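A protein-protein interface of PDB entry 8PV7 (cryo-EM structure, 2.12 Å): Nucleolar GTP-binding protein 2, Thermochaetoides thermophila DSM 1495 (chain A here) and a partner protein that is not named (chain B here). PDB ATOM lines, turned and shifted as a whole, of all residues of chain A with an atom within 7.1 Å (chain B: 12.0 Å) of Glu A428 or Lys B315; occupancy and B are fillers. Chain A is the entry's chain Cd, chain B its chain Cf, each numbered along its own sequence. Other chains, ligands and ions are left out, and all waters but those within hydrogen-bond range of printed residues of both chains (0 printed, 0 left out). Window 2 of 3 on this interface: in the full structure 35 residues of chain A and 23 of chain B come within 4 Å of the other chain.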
ATOM      1  N   HIS A 422       6.799 -32.219  10.681  1.00  0.00           N
ATOM      2  CA  HIS A 422       5.554 -31.795  11.316  1.00  0.00           C
ATOM      3  C   HIS A 422       5.734 -30.474  12.057  1.00  0.00           C
ATOM      4  O   HIS A 422       4.881 -29.587  11.973  1.00  0.00           O
ATOM      5  CB  HIS A 422       5.038 -32.887  12.256  1.00  0.00           C
ATOM      6  CG  HIS A 422       4.538 -34.104  11.545  1.00  0.00           C
ATOM      7  ND1 HIS A 422       4.651 -35.372  12.067  1.00  0.00           N
ATOM      8  CD2 HIS A 422       3.948 -34.247  10.337  1.00  0.00           C
ATOM      9  CE1 HIS A 422       4.132 -36.242  11.221  1.00  0.00           C
ATOM     10  NE2 HIS A 422       3.704 -35.586  10.160  1.00  0.00           N
ATOM     11  N   MET A 423       6.851 -30.325  12.776  1.00  0.00           N
ATOM     12  CA  MET A 423       7.171 -29.058  13.433  1.00  0.00           C
ATOM     13  C   MET A 423       7.349 -27.938  12.415  1.00  0.00           C
ATOM     14  O   MET A 423       6.858 -26.814  12.610  1.00  0.00           O
ATOM     15  CB  MET A 423       8.448 -29.216  14.256  1.00  0.00           C
ATOM     16  CG  MET A 423       8.239 -29.428  15.734  1.00  0.00           C
ATOM     17  SD  MET A 423       7.429 -28.045  16.541  1.00  0.00           S
ATOM     18  CE  MET A 423       7.343 -28.667  18.208  1.00  0.00           C
ATOM     19  N   GLU A 424       8.056 -28.236  11.321  1.00  0.00           N
ATOM     20  CA  GLU A 424       8.312 -27.242  10.286  1.00  0.00           C
ATOM     21  C   GLU A 424       7.023 -26.779   9.626  1.00  0.00           C
ATOM     22  O   GLU A 424       6.856 -25.588   9.356  1.00  0.00           O
ATOM     23  CB  GLU A 424       9.274 -27.804   9.242  1.00  0.00           C
ATOM     24  CG  GLU A 424      10.686 -28.008   9.746  1.00  0.00           C
ATOM     25  CD  GLU A 424      11.538 -28.805   8.787  1.00  0.00           C
ATOM     26  OE1 GLU A 424      10.976 -29.430   7.866  1.00  0.00           O
ATOM     27  OE2 GLU A 424      12.775 -28.807   8.956  1.00  0.00           O
ATOM     28  N   ARG A 425       6.100 -27.701   9.359  1.00  0.00           N
ATOM     29  CA  ARG A 425       4.830 -27.309   8.762  1.00  0.00           C
ATOM     30  C   ARG A 425       3.936 -26.604   9.772  1.00  0.00           C
ATOM     31  O   ARG A 425       3.139 -25.736   9.400  1.00  0.00           O
ATOM     32  CB  ARG A 425       4.126 -28.530   8.179  1.00  0.00           C
ATOM     33  CG  ARG A 425       4.221 -28.631   6.673  1.00  0.00           C
ATOM     34  CD  ARG A 425       4.691 -30.006   6.243  1.00  0.00           C
ATOM     35  NE  ARG A 425       3.748 -31.042   6.641  1.00  0.00           N
ATOM     36  CZ  ARG A 425       3.793 -32.298   6.223  1.00  0.00           C
ATOM     37  NH1 ARG A 425       4.721 -32.711   5.376  1.00  0.00           N
ATOM     38  NH2 ARG A 425       2.883 -33.162   6.663  1.00  0.00           N
ATOM     39  N   THR A 426       4.049 -26.965  11.052  1.00  0.00           N
ATOM     40  CA  THR A 426       3.227 -26.332  12.076  1.00  0.00           C
ATOM     41  C   THR A 426       3.604 -24.869  12.269  1.00  0.00           C
ATOM     42  O   THR A 426       2.727 -24.008  12.392  1.00  0.00           O
ATOM     43  CB  THR A 426       3.356 -27.098  13.392  1.00  0.00           C
ATOM     44  OG1 THR A 426       3.001 -28.467  13.181  1.00  0.00           O
ATOM     45  CG2 THR A 426       2.447 -26.508  14.454  1.00  0.00           C
ATOM     46  N   TYR A 427       4.897 -24.562  12.281  1.00  0.00           N
ATOM     47  CA  TYR A 427       5.319 -23.198  12.576  1.00  0.00           C
ATOM     48  C   TYR A 427       5.863 -22.447  11.367  1.00  0.00           C
ATOM     49  O   TYR A 427       6.266 -21.290  11.517  1.00  0.00           O
ATOM     50  CB  TYR A 427       6.339 -23.206  13.711  1.00  0.00           C
ATOM     51  CG  TYR A 427       5.696 -23.557  15.024  1.00  0.00           C
ATOM     52  CD1 TYR A 427       4.849 -22.664  15.661  1.00  0.00           C
ATOM     53  CD2 TYR A 427       5.907 -24.794  15.608  1.00  0.00           C
ATOM     54  CE1 TYR A 427       4.245 -22.987  16.855  1.00  0.00           C
ATOM     55  CE2 TYR A 427       5.311 -25.125  16.802  1.00  0.00           C
ATOM     56  CZ  TYR A 427       4.479 -24.220  17.419  1.00  0.00           C
ATOM     57  OH  TYR A 427       3.886 -24.556  18.609  1.00  0.00           O
ATOM     58  N   GLU A 428       5.836 -23.056  10.177  1.00  0.00           N
ATOM     59  CA  GLU A 428       6.352 -22.479   8.928  1.00  0.00           C
ATOM     60  C   GLU A 428       7.787 -21.977   9.091  1.00  0.00           C
ATOM     61  O   GLU A 428       8.141 -20.870   8.685  1.00  0.00           O
ATOM     62  CB  GLU A 428       5.432 -21.376   8.405  1.00  0.00           C
ATOM     63  CG  GLU A 428       4.233 -21.883   7.632  1.00  0.00           C
ATOM     64  CD  GLU A 428       2.930 -21.287   8.117  1.00  0.00           C
ATOM     65  OE1 GLU A 428       2.967 -20.417   9.011  1.00  0.00           O
ATOM     66  OE2 GLU A 428       1.865 -21.683   7.599  1.00  0.00           O
ATOM     67  N   LEU A 429       8.615 -22.813   9.706  1.00  0.00           N
ATOM     68  CA  LEU A 429       9.971 -22.454  10.082  1.00  0.00           C
ATOM     69  C   LEU A 429      10.880 -23.639   9.806  1.00  0.00           C
ATOM     70  O   LEU A 429      10.468 -24.791   9.933  1.00  0.00           O
ATOM     71  CB  LEU A 429      10.029 -22.058  11.560  1.00  0.00           C
ATOM     72  CG  LEU A 429      11.210 -21.259  12.086  1.00  0.00           C
ATOM     73  CD1 LEU A 429      11.064 -19.802  11.703  1.00  0.00           C
ATOM     74  CD2 LEU A 429      11.299 -21.418  13.588  1.00  0.00           C
ATOM     75  N   ARG A 430      12.127 -23.360   9.436  1.00  0.00           N
ATOM     76  CA  ARG A 430      13.065 -24.443   9.166  1.00  0.00           C
ATOM     77  C   ARG A 430      14.490 -23.948   9.342  1.00  0.00           C
ATOM     78  O   ARG A 430      14.761 -22.746   9.307  1.00  0.00           O
ATOM     79  CB  ARG A 430      12.875 -25.018   7.759  1.00  0.00           C
ATOM     80  CG  ARG A 430      12.819 -23.974   6.667  1.00  0.00           C
ATOM     81  CD  ARG A 430      11.950 -24.441   5.517  1.00  0.00           C
ATOM     82  NE  ARG A 430      10.698 -25.022   5.989  1.00  0.00           N
ATOM     83  CZ  ARG A 430       9.582 -24.336   6.192  1.00  0.00           C
ATOM     84  NH1 ARG A 430       9.525 -23.031   5.979  1.00  0.00           N
ATOM     85  NH2 ARG A 430       8.496 -24.972   6.621  1.00  0.00           N
ATOM     86  N   TRP A 432      16.809 -24.911  11.973  1.00  0.00           N
ATOM     87  CA  TRP A 432      17.425 -24.843  13.288  1.00  0.00           C
ATOM     88  C   TRP A 432      18.250 -26.096  13.550  1.00  0.00           C
ATOM     89  O   TRP A 432      17.932 -27.185  13.066  1.00  0.00           O
ATOM     90  CB  TRP A 432      16.365 -24.677  14.380  1.00  0.00           C
ATOM     91  CG  TRP A 432      15.415 -25.835  14.521  1.00  0.00           C
ATOM     92  CD1 TRP A 432      15.600 -26.960  15.269  1.00  0.00           C
ATOM     93  CD2 TRP A 432      14.128 -25.970  13.911  1.00  0.00           C
ATOM     94  NE1 TRP A 432      14.516 -27.788  15.156  1.00  0.00           N
ATOM     95  CE2 TRP A 432      13.597 -27.205  14.327  1.00  0.00           C
ATOM     96  CE3 TRP A 432      13.373 -25.167  13.053  1.00  0.00           C
ATOM     97  CZ2 TRP A 432      12.348 -27.657  13.915  1.00  0.00           C
ATOM     98  CZ3 TRP A 432      12.135 -25.617  12.644  1.00  0.00           C
ATOM     99  CH2 TRP A 432      11.634 -26.850  13.075  1.00  0.00           C
ATOM    100  N   LEU A 442      11.549 -18.820  16.253  1.00  0.00           N
ATOM    101  CA  LEU A 442      10.104 -18.704  16.417  1.00  0.00           C
ATOM    102  C   LEU A 442       9.726 -17.396  17.110  1.00  0.00           C
ATOM    103  O   LEU A 442       8.742 -16.750  16.730  1.00  0.00           O
ATOM    104  CB  LEU A 442       9.562 -19.910  17.184  1.00  0.00           C
ATOM    105  CG  LEU A 442       8.037 -20.029  17.263  1.00  0.00           C
ATOM    106  CD1 LEU A 442       7.392 -19.773  15.912  1.00  0.00           C
ATOM    107  CD2 LEU A 442       7.620 -21.385  17.802  1.00  0.00           C
ATOM    108  N   LYS A 445      10.177 -14.530  14.623  1.00  0.00           N
ATOM    109  CA  LYS A 445       9.150 -14.563  13.592  1.00  0.00           C
ATOM    110  C   LYS A 445       7.802 -14.104  14.134  1.00  0.00           C
ATOM    111  O   LYS A 445       7.089 -13.341  13.474  1.00  0.00           O
ATOM    112  CB  LYS A 445       9.043 -15.970  13.016  1.00  0.00           C
ATOM    113  CG  LYS A 445       7.996 -16.104  11.951  1.00  0.00           C
ATOM    114  CD  LYS A 445       7.699 -17.549  11.674  1.00  0.00           C
ATOM    115  CE  LYS A 445       6.514 -17.672  10.753  1.00  0.00           C
ATOM    116  NZ  LYS A 445       6.088 -19.077  10.644  1.00  0.00           N
ATOM    117  N   LYS A 472      -2.390 -29.275  18.909  1.00  0.00           N
ATOM    118  CA  LYS A 472      -2.116 -28.389  17.790  1.00  0.00           C
ATOM    119  C   LYS A 472      -0.856 -28.764  17.026  1.00  0.00           C
ATOM    120  O   LYS A 472      -0.618 -28.210  15.952  1.00  0.00           O
ATOM    121  CB  LYS A 472      -2.013 -26.937  18.273  1.00  0.00           C
ATOM    122  CG  LYS A 472      -3.323 -26.399  18.821  1.00  0.00           C
ATOM    123  CD  LYS A 472      -3.229 -24.926  19.141  1.00  0.00           C
ATOM    124  CE  LYS A 472      -4.575 -24.363  19.541  1.00  0.00           C
ATOM    125  NZ  LYS A 472      -5.156 -25.103  20.687  1.00  0.00           N
ATOM    126  N   ILE A 473      -0.055 -29.684  17.553  1.00  0.00           N
ATOM    127  CA  ILE A 473       1.095 -30.246  16.861  1.00  0.00           C
ATOM    128  C   ILE A 473       0.864 -31.745  16.745  1.00  0.00           C
ATOM    129  O   ILE A 473       0.566 -32.391  17.750  1.00  0.00           O
ATOM    130  CB  ILE A 473       2.420 -29.966  17.593  1.00  0.00           C
ATOM    131  CG1 ILE A 473       2.507 -28.499  18.009  1.00  0.00           C
ATOM    132  CG2 ILE A 473       3.589 -30.328  16.715  1.00  0.00           C
ATOM    133  CD1 ILE A 473       3.652 -28.194  18.939  1.00  0.00           C
ATOM    134  N   PRO A 474       0.969 -32.337  15.557  1.00  0.00           N
ATOM    135  CA  PRO A 474       0.681 -33.773  15.421  1.00  0.00           C
ATOM    136  C   PRO A 474       1.795 -34.639  15.993  1.00  0.00           C
ATOM    137  O   PRO A 474       2.971 -34.457  15.672  1.00  0.00           O
ATOM    138  CB  PRO A 474       0.544 -33.963  13.908  1.00  0.00           C
ATOM    139  CG  PRO A 474       1.307 -32.841  13.317  1.00  0.00           C
ATOM    140  CD  PRO A 474       1.162 -31.687  14.251  1.00  0.00           C
ATOM    141  N   THR B 311      -9.969 -37.915  10.870  1.00  0.00           N
ATOM    142  CA  THR B 311      -8.998 -37.393  11.813  1.00  0.00           C
ATOM    143  C   THR B 311      -8.916 -35.877  11.687  1.00  0.00           C
ATOM    144  O   THR B 311      -9.352 -35.286  10.698  1.00  0.00           O
ATOM    145  CB  THR B 311      -7.627 -38.027  11.588  1.00  0.00           C
ATOM    146  OG1 THR B 311      -7.273 -37.942  10.205  1.00  0.00           O
ATOM    147  CG2 THR B 311      -7.674 -39.479  11.986  1.00  0.00           C
ATOM    148  N   ARG B 312      -8.374 -35.245  12.722  1.00  0.00           N
ATOM    149  CA  ARG B 312      -8.299 -33.792  12.752  1.00  0.00           C
ATOM    150  C   ARG B 312      -7.317 -33.285  11.708  1.00  0.00           C
ATOM    151  O   ARG B 312      -6.184 -33.766  11.618  1.00  0.00           O
ATOM    152  CB  ARG B 312      -7.890 -33.319  14.144  1.00  0.00           C
ATOM    153  CG  ARG B 312      -7.925 -31.820  14.327  1.00  0.00           C
ATOM    154  CD  ARG B 312      -7.771 -31.449  15.785  1.00  0.00           C
ATOM    155  NE  ARG B 312      -7.947 -30.021  16.013  1.00  0.00           N
ATOM    156  CZ  ARG B 312      -9.119 -29.430  16.198  1.00  0.00           C
ATOM    157  NH1 ARG B 312     -10.249 -30.115  16.178  1.00  0.00           N
ATOM    158  NH2 ARG B 312      -9.159 -28.120  16.409  1.00  0.00           N
ATOM    159  N   LYS B 313      -7.754 -32.305  10.918  1.00  0.00           N
ATOM    160  CA  LYS B 313      -6.934 -31.747   9.845  1.00  0.00           C
ATOM    161  C   LYS B 313      -6.007 -30.685  10.435  1.00  0.00           C
ATOM    162  O   LYS B 313      -6.209 -29.478  10.305  1.00  0.00           O
ATOM    163  CB  LYS B 313      -7.807 -31.176   8.738  1.00  0.00           C
ATOM    164  CG  LYS B 313      -8.929 -32.087   8.284  1.00  0.00           C
ATOM    165  CD  LYS B 313      -8.423 -33.450   7.870  1.00  0.00           C
ATOM    166  CE  LYS B 313      -9.583 -34.373   7.564  1.00  0.00           C
ATOM    167  NZ  LYS B 313      -9.156 -35.785   7.490  1.00  0.00           N
ATOM    168  N   MET B 314      -4.971 -31.170  11.110  1.00  0.00           N
ATOM    169  CA  MET B 314      -4.030 -30.287  11.773  1.00  0.00           C
ATOM    170  C   MET B 314      -3.154 -29.560  10.760  1.00  0.00           C
ATOM    171  O   MET B 314      -2.973 -30.003   9.624  1.00  0.00           O
ATOM    172  CB  MET B 314      -3.167 -31.075  12.754  1.00  0.00           C
ATOM    173  CG  MET B 314      -3.947 -31.612  13.937  1.00  0.00           C
ATOM    174  SD  MET B 314      -2.916 -32.384  15.193  1.00  0.00           S
ATOM    175  CE  MET B 314      -3.220 -34.109  14.847  1.00  0.00           C
ATOM    176  N   LYS B 315      -2.624 -28.415  11.192  1.00  0.00           N
ATOM    177  CA  LYS B 315      -1.801 -27.578  10.326  1.00  0.00           C
ATOM    178  C   LYS B 315      -0.507 -28.279   9.935  1.00  0.00           C
ATOM    179  O   LYS B 315      -0.013 -28.108   8.817  1.00  0.00           O
ATOM    180  CB  LYS B 315      -1.511 -26.256  11.036  1.00  0.00           C
ATOM    181  CG  LYS B 315      -0.803 -25.209  10.212  1.00  0.00           C
ATOM    182  CD  LYS B 315      -0.474 -24.011  11.083  1.00  0.00           C
ATOM    183  CE  LYS B 315       0.036 -22.845  10.267  1.00  0.00           C
ATOM    184  NZ  LYS B 315       0.449 -21.717  11.141  1.00  0.00           N
ATOM    185  N   GLY B 316       0.052 -29.080  10.843  1.00  0.00           N
ATOM    186  CA  GLY B 316       1.293 -29.777  10.563  1.00  0.00           C
ATOM    187  C   GLY B 316       1.156 -30.934   9.600  1.00  0.00           C
ATOM    188  O   GLY B 316       2.165 -31.401   9.066  1.00  0.00           O
ATOM    189  N   LEU B 317      -0.063 -31.413   9.369  1.00  0.00           N
ATOM    190  CA  LEU B 317      -0.306 -32.507   8.443  1.00  0.00           C
ATOM    191  C   LEU B 317      -0.671 -32.032   7.046  1.00  0.00           C
ATOM    192  O   LEU B 317      -0.931 -32.863   6.175  1.00  0.00           O
ATOM    193  CB  LEU B 317      -1.411 -33.417   8.980  1.00  0.00           C
ATOM    194  CG  LEU B 317      -1.113 -34.148  10.286  1.00  0.00           C
ATOM    195  CD1 LEU B 317      -2.300 -34.992  10.691  1.00  0.00           C
ATOM    196  CD2 LEU B 317       0.136 -34.997  10.150  1.00  0.00           C
ATOM    197  N   LYS B 318      -0.695 -30.726   6.809  1.00  0.00           N
ATOM    198  CA  LYS B 318      -1.031 -30.169   5.507  1.00  0.00           C
ATOM    199  C   LYS B 318       0.257 -29.857   4.758  1.00  0.00           C
ATOM    200  O   LYS B 318       1.221 -29.363   5.352  1.00  0.00           O
ATOM    201  CB  LYS B 318      -1.896 -28.920   5.655  1.00  0.00           C
ATOM    202  CG  LYS B 318      -3.217 -29.187   6.345  1.00  0.00           C
ATOM    203  CD  LYS B 318      -4.025 -27.922   6.539  1.00  0.00           C
ATOM    204  CE  LYS B 318      -5.384 -28.238   7.138  1.00  0.00           C
ATOM    205  NZ  LYS B 318      -6.192 -27.014   7.372  1.00  0.00           N
ATOM    206  N   ARG B 319       0.273 -30.156   3.465  1.00  0.00           N
ATOM    207  CA  ARG B 319       1.478 -30.030   2.651  1.00  0.00           C
ATOM    208  C   ARG B 319       1.793 -28.560   2.393  1.00  0.00           C
ATOM    209  O   ARG B 319       0.992 -27.839   1.800  1.00  0.00           O
ATOM    210  CB  ARG B 319       1.363 -30.775   1.300  1.00  0.00           C
ATOM    211  CG  ARG B 319       1.176 -32.331   1.253  1.00  0.00           C
ATOM    212  CD  ARG B 319       0.089 -32.966   2.126  1.00  0.00           C
ATOM    213  NE  ARG B 319      -1.223 -32.384   1.867  1.00  0.00           N
ATOM    214  CZ  ARG B 319      -2.301 -32.595   2.610  1.00  0.00           C
ATOM    215  NH1 ARG B 319      -2.262 -33.372   3.678  1.00  0.00           N
ATOM    216  NH2 ARG B 319      -3.446 -32.008   2.274  1.00  0.00           N
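Of chain B, only Lys B315 (3.5 Å) and Gly B316 (3.4 Å) come within 4 Å of Thr A426.
No residue of chain B comes within 4 Å of Leu A429.
Of the printed residues of chain B, His A422 touches Gly B316 and Leu B317.
Printed residues of chain A within 4 Å of Gly B316: His A422, Arg A425 and Thr A426.
Of the printed residues of chain A, Met B314 touches Pro A474 (3.9 Å).
The nearest residue of chain B that does not touch Glu A428 is Lys B318 (8.0 Å).
The nearest printed residue of chain B that does not touch His A422 is Lys B315 (5.9 Å).
Of the 15 printed residues of chain A, 5 touch a printed residue of chain B.
Printed residues of chain A that touch a printed residue of chain B: His A422, Arg A425, Thr A426, Glu A428 and Pro A474.
Of the 9 printed residues of chain B, 5 touch a printed residue of chain A.
Hydrophobic or aromatic side chains of chain B that line the printed part of chain A: Met B314 and Leu B317.
Among the printed residues, Asp or Glu carboxylates within 4 Å of a Lys or Arg side-chain nitrogen of the other chain: Glu A428 with Lys B315 (3.5 Å).
NE of Arg A425 is in hydrogen-bond range of O of Gly B316 (2.9 Å).
NE of Arg A425 sits at hydrogen-bond distance from O of Lys B318, 3.3 Å away.
O of Thr A426 sits close to NZ of Lys B315.
The side-chain carboxylate (OE1) of Glu A428 is in salt-bridge range of the side-chain amino group (NZ) of Lys B315, at 3.5 Å.
The backbone carbonyl oxygen (O) of His A422 sits at hydrogen-bond distance from the side-chain hydroxyl (OG1) of Thr A426 (2.5 Å).
The side-chain amino group (NZ) of Lys A445 lies within salt-bridge range of the side-chain carboxylate (OE1) of Glu A428.
The backbone carbonyl oxygen of Leu B317 is in hydrogen-bond range of the guanidinium group of Arg B319 (2.9 Å).
Among the printed residues, pairs that only touch across the chains: His A422 with Gly B316 (3.6 Å), His A422 with Leu B317 (3.6 Å), Arg A425 with Lys B315 (3.99 Å), Arg A425 with Leu B317 (3.7 Å), Thr A426 with Gly B316 (3.4 Å), Pro A474 with Met B314 (3.9 Å) and Pro A474 with Leu B317 (3.9 Å).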
